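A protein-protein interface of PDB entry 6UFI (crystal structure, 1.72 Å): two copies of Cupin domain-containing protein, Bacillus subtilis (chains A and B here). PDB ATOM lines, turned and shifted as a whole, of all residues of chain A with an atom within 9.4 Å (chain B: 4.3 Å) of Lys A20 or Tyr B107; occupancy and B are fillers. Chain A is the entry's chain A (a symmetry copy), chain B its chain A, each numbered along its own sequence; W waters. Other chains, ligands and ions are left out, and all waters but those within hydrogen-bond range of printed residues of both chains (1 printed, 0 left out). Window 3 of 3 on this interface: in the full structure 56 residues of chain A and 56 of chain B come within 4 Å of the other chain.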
ATOM      1  N   PRO A   8     -17.628 -32.221  21.556  1.00  0.00           N
ATOM      2  CA  PRO A   8     -18.202 -30.915  21.894  1.00  0.00           C
ATOM      3  C   PRO A   8     -17.236 -30.077  22.720  1.00  0.00           C
ATOM      4  O   PRO A   8     -16.404 -30.598  23.466  1.00  0.00           O
ATOM      5  CB  PRO A   8     -19.455 -31.273  22.697  1.00  0.00           C
ATOM      6  CG  PRO A   8     -19.106 -32.580  23.335  1.00  0.00           C
ATOM      7  CD  PRO A   8     -18.257 -33.315  22.320  1.00  0.00           C
ATOM      8  N   GLN A   9     -17.353 -28.758  22.567  1.00  0.00           N
ATOM      9  CA  GLN A   9     -16.507 -27.833  23.305  1.00  0.00           C
ATOM     10  C   GLN A   9     -17.349 -26.769  23.988  1.00  0.00           C
ATOM     11  O   GLN A   9     -18.399 -26.363  23.469  1.00  0.00           O
ATOM     12  CB  GLN A   9     -15.493 -27.139  22.382  1.00  0.00           C
ATOM     13  CG  GLN A   9     -14.543 -28.118  21.711  1.00  0.00           C
ATOM     14  CD  GLN A   9     -13.509 -28.690  22.659  1.00  0.00           C
ATOM     15  OE1 GLN A   9     -13.443 -28.318  23.836  1.00  0.00           O
ATOM     16  NE2 GLN A   9     -12.683 -29.606  22.150  1.00  0.00           N
ATOM     17  N   PRO A  10     -16.898 -26.282  25.147  1.00  0.00           N
ATOM     18  CA  PRO A  10     -17.618 -25.196  25.846  1.00  0.00           C
ATOM     19  C   PRO A  10     -17.330 -23.843  25.210  1.00  0.00           C
ATOM     20  O   PRO A  10     -16.641 -22.979  25.762  1.00  0.00           O
ATOM     21  CB  PRO A  10     -17.085 -25.314  27.278  1.00  0.00           C
ATOM     22  CG  PRO A  10     -15.709 -25.914  27.120  1.00  0.00           C
ATOM     23  CD  PRO A  10     -15.782 -26.833  25.936  1.00  0.00           C
ATOM     24  N   ALA A  17     -13.971 -21.632  25.510  1.00  0.00           N
ATOM     25  CA  ALA A  17     -12.699 -22.102  24.952  1.00  0.00           C
ATOM     26  C   ALA A  17     -12.722 -23.625  24.884  1.00  0.00           C
ATOM     27  O   ALA A  17     -13.602 -24.272  25.451  1.00  0.00           O
ATOM     28  CB  ALA A  17     -11.505 -21.634  25.794  1.00  0.00           C
ATOM     29  N   THR A  18     -11.739 -24.195  24.181  1.00  0.00           N
ATOM     30  CA  THR A  18     -11.629 -25.651  24.147  1.00  0.00           C
ATOM     31  C   THR A  18     -11.152 -26.185  25.493  1.00  0.00           C
ATOM     32  O   THR A  18     -10.458 -25.494  26.251  1.00  0.00           O
ATOM     33  CB  THR A  18     -10.662 -26.106  23.054  1.00  0.00           C
ATOM     34  OG1 THR A  18      -9.400 -25.455  23.243  1.00  0.00           O
ATOM     35  CG2 THR A  18     -11.231 -25.776  21.691  1.00  0.00           C
ATOM     36  N   VAL A  19     -11.545 -27.421  25.802  1.00  0.00           N
ATOM     37  CA  VAL A  19     -11.062 -28.080  27.014  1.00  0.00           C
ATOM     38  C   VAL A  19      -9.654 -28.599  26.755  1.00  0.00           C
ATOM     39  O   VAL A  19      -9.412 -29.305  25.770  1.00  0.00           O
ATOM     40  CB  VAL A  19     -12.003 -29.224  27.436  1.00  0.00           C
ATOM     41  CG1 VAL A  19     -11.500 -29.843  28.743  1.00  0.00           C
ATOM     42  CG2 VAL A  19     -13.417 -28.708  27.636  1.00  0.00           C
ATOM     43  N   LYS A  20      -8.717 -28.254  27.646  1.00  0.00           N
ATOM     44  CA  LYS A  20      -7.318 -28.617  27.462  1.00  0.00           C
ATOM     45  C   LYS A  20      -6.848 -29.731  28.390  1.00  0.00           C
ATOM     46  O   LYS A  20      -5.734 -30.235  28.203  1.00  0.00           O
ATOM     47  CB  LYS A  20      -6.410 -27.395  27.672  1.00  0.00           C
ATOM     48  CG  LYS A  20      -6.502 -26.349  26.568  1.00  0.00           C
ATOM     49  CD  LYS A  20      -5.826 -26.837  25.292  1.00  0.00           C
ATOM     50  CE  LYS A  20      -5.725 -25.708  24.274  1.00  0.00           C
ATOM     51  NZ  LYS A  20      -5.068 -26.253  23.035  1.00  0.00           N
ATOM     52  N   ILE A  21      -7.644 -30.117  29.382  1.00  0.00           N
ATOM     53  CA  ILE A  21      -7.271 -31.148  30.350  1.00  0.00           C
ATOM     54  C   ILE A  21      -8.025 -32.432  30.028  1.00  0.00           C
ATOM     55  O   ILE A  21      -8.995 -32.399  29.248  1.00  0.00           O
ATOM     56  CB  ILE A  21      -7.567 -30.678  31.786  1.00  0.00           C
ATOM     57  CG1 ILE A  21      -9.068 -30.435  31.970  1.00  0.00           C
ATOM     58  CG2 ILE A  21      -6.790 -29.406  32.078  1.00  0.00           C
ATOM     59  CD1 ILE A  21      -9.474 -30.072  33.418  1.00  0.00           C
ATOM     60  N   PRO A  22      -7.625 -33.574  30.598  1.00  0.00           N
ATOM     61  CA  PRO A  22      -8.407 -34.797  30.408  1.00  0.00           C
ATOM     62  C   PRO A  22      -9.834 -34.614  30.907  1.00  0.00           C
ATOM     63  O   PRO A  22     -10.084 -33.932  31.904  1.00  0.00           O
ATOM     64  CB  PRO A  22      -7.643 -35.843  31.227  1.00  0.00           C
ATOM     65  CG  PRO A  22      -6.233 -35.338  31.254  1.00  0.00           C
ATOM     66  CD  PRO A  22      -6.391 -33.830  31.369  1.00  0.00           C
ATOM     67  N   ARG A  23     -10.777 -35.218  30.187  1.00  0.00           N
ATOM     68  CA  ARG A  23     -12.185 -34.893  30.382  1.00  0.00           C
ATOM     69  C   ARG A  23     -13.062 -36.114  30.145  1.00  0.00           C
ATOM     70  O   ARG A  23     -12.615 -37.147  29.642  1.00  0.00           O
ATOM     71  CB  ARG A  23     -12.610 -33.760  29.441  1.00  0.00           C
ATOM     72  CG  ARG A  23     -12.426 -34.144  27.982  1.00  0.00           C
ATOM     73  CD  ARG A  23     -12.646 -32.993  27.008  1.00  0.00           C
ATOM     74  NE  ARG A  23     -14.031 -32.554  27.019  1.00  0.00           N
ATOM     75  CZ  ARG A  23     -14.611 -31.889  26.024  1.00  0.00           C
ATOM     76  NH1 ARG A  23     -13.919 -31.591  24.927  1.00  0.00           N
ATOM     77  NH2 ARG A  23     -15.884 -31.535  26.126  1.00  0.00           N
ATOM     78  N   ASP A  28     -20.142 -35.140  28.824  1.00  0.00           N
ATOM     79  CA  ASP A  28     -20.356 -33.861  28.152  1.00  0.00           C
ATOM     80  C   ASP A  28     -21.409 -33.991  27.055  1.00  0.00           C
ATOM     81  O   ASP A  28     -22.238 -33.095  26.871  1.00  0.00           O
ATOM     82  CB  ASP A  28     -19.047 -33.325  27.557  1.00  0.00           C
ATOM     83  CG  ASP A  28     -18.071 -32.817  28.617  1.00  0.00           C
ATOM     84  OD1 ASP A  28     -18.486 -32.585  29.775  1.00  0.00           O
ATOM     85  OD2 ASP A  28     -16.877 -32.642  28.290  1.00  0.00           O
ATOM     86  N   ARG B  85     -10.482 -22.089  33.094  1.00  0.00           N
ATOM     87  CA  ARG B  85      -9.744 -22.096  31.836  1.00  0.00           C
ATOM     88  C   ARG B  85      -9.577 -20.666  31.350  1.00  0.00           C
ATOM     89  O   ARG B  85     -10.545 -19.896  31.330  1.00  0.00           O
ATOM     90  CB  ARG B  85     -10.487 -22.925  30.793  1.00  0.00           C
ATOM     91  CG  ARG B  85     -10.030 -22.725  29.342  1.00  0.00           C
ATOM     92  CD  ARG B  85      -8.810 -23.564  29.012  1.00  0.00           C
ATOM     93  NE  ARG B  85      -8.791 -23.853  27.570  1.00  0.00           N
ATOM     94  CZ  ARG B  85      -8.089 -23.184  26.663  1.00  0.00           C
ATOM     95  NH1 ARG B  85      -7.295 -22.187  27.025  1.00  0.00           N
ATOM     96  NH2 ARG B  85      -8.182 -23.528  25.378  1.00  0.00           N
ATOM     97  N   MET B 105      -1.724 -26.257  38.612  1.00  0.00           N
ATOM     98  CA  MET B 105      -1.705 -25.935  37.183  1.00  0.00           C
ATOM     99  C   MET B 105      -1.631 -27.234  36.384  1.00  0.00           C
ATOM    100  O   MET B 105      -0.598 -27.913  36.371  1.00  0.00           O
ATOM    101  CB  MET B 105      -0.541 -24.997  36.858  1.00  0.00           C
ATOM    102  CG  MET B 105      -0.521 -24.444  35.401  1.00  0.00           C
ATOM    103  SD  MET B 105      -1.965 -23.435  34.906  1.00  0.00           S
ATOM    104  CE  MET B 105      -1.856 -22.003  35.976  1.00  0.00           C
ATOM    105  N   ILE B 106      -2.735 -27.583  35.721  1.00  0.00           N
ATOM    106  CA  ILE B 106      -2.792 -28.822  34.940  1.00  0.00           C
ATOM    107  C   ILE B 106      -2.231 -28.628  33.539  1.00  0.00           C
ATOM    108  O   ILE B 106      -1.484 -29.483  33.042  1.00  0.00           O
ATOM    109  CB  ILE B 106      -4.235 -29.356  34.873  1.00  0.00           C
ATOM    110  CG1 ILE B 106      -4.820 -29.500  36.278  1.00  0.00           C
ATOM    111  CG2 ILE B 106      -4.271 -30.695  34.107  1.00  0.00           C
ATOM    112  CD1 ILE B 106      -6.327 -29.749  36.248  1.00  0.00           C
ATOM    113  N   TYR B 107      -2.601 -27.526  32.887  1.00  0.00           N
ATOM    114  CA  TYR B 107      -2.226 -27.241  31.510  1.00  0.00           C
ATOM    115  C   TYR B 107      -1.747 -25.799  31.387  1.00  0.00           C
ATOM    116  O   TYR B 107      -2.350 -24.886  31.951  1.00  0.00           O
ATOM    117  CB  TYR B 107      -3.409 -27.477  30.537  1.00  0.00           C
ATOM    118  CG  TYR B 107      -3.134 -26.826  29.202  1.00  0.00           C
ATOM    119  CD1 TYR B 107      -2.372 -27.484  28.252  1.00  0.00           C
ATOM    120  CD2 TYR B 107      -3.587 -25.541  28.918  1.00  0.00           C
ATOM    121  CE1 TYR B 107      -2.072 -26.885  27.047  1.00  0.00           C
ATOM    122  CE2 TYR B 107      -3.288 -24.929  27.699  1.00  0.00           C
ATOM    123  CZ  TYR B 107      -2.533 -25.615  26.776  1.00  0.00           C
ATOM    124  OH  TYR B 107      -2.213 -25.028  25.565  1.00  0.00           O
ATOM    125  N   GLY B 108      -0.672 -25.588  30.629  1.00  0.00           N
ATOM    126  CA  GLY B 108      -0.305 -24.229  30.262  1.00  0.00           C
ATOM    127  C   GLY B 108       0.486 -23.496  31.339  1.00  0.00           C
ATOM    128  O   GLY B 108       1.271 -24.083  32.088  1.00  0.00           O
ATOM    129  N   SER B 109       0.274 -22.184  31.415  1.00  0.00           N
ATOM    130  CA  SER B 109       1.025 -21.366  32.365  1.00  0.00           C
ATOM    131  C   SER B 109       0.303 -20.044  32.570  1.00  0.00           C
ATOM    132  O   SER B 109      -0.513 -19.629  31.747  1.00  0.00           O
ATOM    133  CB  SER B 109       2.467 -21.125  31.891  1.00  0.00           C
ATOM    134  OG  SER B 109       2.513 -20.405  30.663  1.00  0.00           O
ATOM    135  N   GLU B 128       2.999 -25.911  34.381  1.00  0.00           N
ATOM    136  CA  GLU B 128       2.382 -27.210  34.664  1.00  0.00           C
ATOM    137  C   GLU B 128       3.081 -27.891  35.832  1.00  0.00           C
ATOM    138  O   GLU B 128       4.314 -27.966  35.884  1.00  0.00           O
ATOM    139  CB  GLU B 128       2.413 -28.110  33.418  1.00  0.00           C
ATOM    140  CG  GLU B 128       1.410 -27.662  32.356  1.00  0.00           C
ATOM    141  CD  GLU B 128       1.591 -28.355  31.014  1.00  0.00           C
ATOM    142  OE1 GLU B 128       2.314 -29.377  30.964  1.00  0.00           O
ATOM    143  OE2 GLU B 128       1.005 -27.873  30.010  1.00  0.00           O
ATOM    144  N   GLU B 147       0.394 -20.081  26.038  1.00  0.00           N
ATOM    145  CA  GLU B 147      -0.306 -21.331  25.778  1.00  0.00           C
ATOM    146  C   GLU B 147      -1.726 -21.342  26.329  1.00  0.00           C
ATOM    147  O   GLU B 147      -2.443 -22.330  26.119  1.00  0.00           O
ATOM    148  CB  GLU B 147       0.476 -22.516  26.365  1.00  0.00           C
ATOM    149  CG  GLU B 147       1.817 -22.780  25.663  1.00  0.00           C
ATOM    150  CD  GLU B 147       1.653 -23.242  24.224  1.00  0.00           C
ATOM    151  OE1 GLU B 147       0.649 -23.915  23.914  1.00  0.00           O
ATOM    152  OE2 GLU B 147       2.538 -22.935  23.399  1.00  0.00           O
ATOM    153  N   GLY B 148      -2.160 -20.262  26.992  1.00  0.00           N
ATOM    154  CA  GLY B 148      -3.380 -20.334  27.782  1.00  0.00           C
ATOM    155  C   GLY B 148      -3.091 -21.110  29.069  1.00  0.00           C
ATOM    156  O   GLY B 148      -1.953 -21.460  29.379  1.00  0.00           O
ATOM    157  N   ALA B 149      -4.155 -21.392  29.823  1.00  0.00           N
ATOM    158  CA  ALA B 149      -3.971 -22.112  31.079  1.00  0.00           C
ATOM    159  C   ALA B 149      -5.264 -22.812  31.454  1.00  0.00           C
ATOM    160  O   ALA B 149      -6.354 -22.319  31.164  1.00  0.00           O
ATOM    161  CB  ALA B 149      -3.548 -21.161  32.210  1.00  0.00           C
ATOM    162  N   GLU B 150      -5.138 -23.973  32.097  1.00  0.00           N
ATOM    163  CA  GLU B 150      -6.300 -24.601  32.710  1.00  0.00           C
ATOM    164  C   GLU B 150      -5.855 -25.217  34.026  1.00  0.00           C
ATOM    165  O   GLU B 150      -4.828 -25.897  34.084  1.00  0.00           O
ATOM    166  CB  GLU B 150      -6.948 -25.658  31.793  1.00  0.00           C
ATOM    167  CG  GLU B 150      -8.279 -26.166  32.386  1.00  0.00           C
ATOM    168  CD  GLU B 150      -9.241 -26.769  31.373  1.00  0.00           C
ATOM    169  OE1 GLU B 150      -8.836 -27.006  30.211  1.00  0.00           O
ATOM    170  OE2 GLU B 150     -10.421 -27.000  31.737  1.00  0.00           O
HETATM  171  O   HOH W   1      -2.333 -26.664  23.123  1.00  0.00           O
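OE1 of Glu B150 sits at hydrogen-bond distance from N of Ile A21 (3.4 Å). The guanidinium group (NE) of Arg B85 lies within hydrogen-bond range of the backbone carbonyl oxygen (O) of Thr A18 (2.7 Å). The backbone NH of Lys A20 sits at hydrogen-bond distance from the side-chain carboxylate of Glu B150, 2.9 Å away.
The backbone NH of Val A19 sits at hydrogen-bond distance from the side-chain amide oxygen of Gln A9 (2.9 Å). The backbone carbonyl oxygen of Tyr B107 sits at hydrogen-bond distance from the backbone NH of Glu B150 (2.9 Å). O of Glu B147 is in hydrogen-bond range of OH of Tyr B107. The backbone carbonyl oxygen (O) of Pro A10 lies within hydrogen-bond range of the backbone NH (N) of Ala A17 (3.0 Å). N of Ile B106 sits at hydrogen-bond distance from O of Glu B150 (3.1 Å).
Among the printed residues, pairs that only touch across the chains: Lys A20 with Arg B85, Ile A21 with Ile B106, Lys A20 with Tyr B107, Ala A17 with Arg B85 and Val A19 with Glu B150.
Of the printed residues of chain B, Ala A17 touches Arg B85. Of the printed residues of chain B, Thr A18 touches Arg B85 (2.7 Å). Of the printed residues of chain B, Val A19 touches Glu B150 (3.9 Å). Lys A20 touches just these residues of chain B: Arg B85, Tyr B107 and Glu B150. Printed residues of chain B within 4 Å of Ile A21: Ile B106 and Glu B150. Of the printed residues of chain A, Ile B106 touches Ile A21. Tyr B107 touches just one residue of chain A: Lys A20. No residue of chain A comes within 4 Å of Gly B148. No residue of chain A comes within 4 Å of Ala B149. The nearest printed residue of chain B that does not touch Lys A20 is Glu B147 (5.1 Å). The nearest printed residue of chain A that does not touch Ile B106 is Pro A22 (4.7 Å).
Hydrophobic or aromatic side chains of chain B that line the printed part of chain A: Ile B106 and Tyr B107. Printed residues of chain A that touch a printed residue of chain B: Ala A17, Thr A18, Val A19, Lys A20 and Ile A21. Among the printed residues, 8 pairs touch across the chains. Among the printed residues, no Asp or Glu carboxylate lies within 4 Å of a Lys or Arg side-chain nitrogen of the other chain.
No position is printed for both chains. Of the 8 pairs that touch across the chains among the printed residues, none has its exchanged pair printed and touching as well.
Water W1 lies within hydrogen-bond range of the side-chain amino group of Lys A20 (2.8 Å) and the side-chain hydroxyl of Tyr B107 (2.9 Å).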
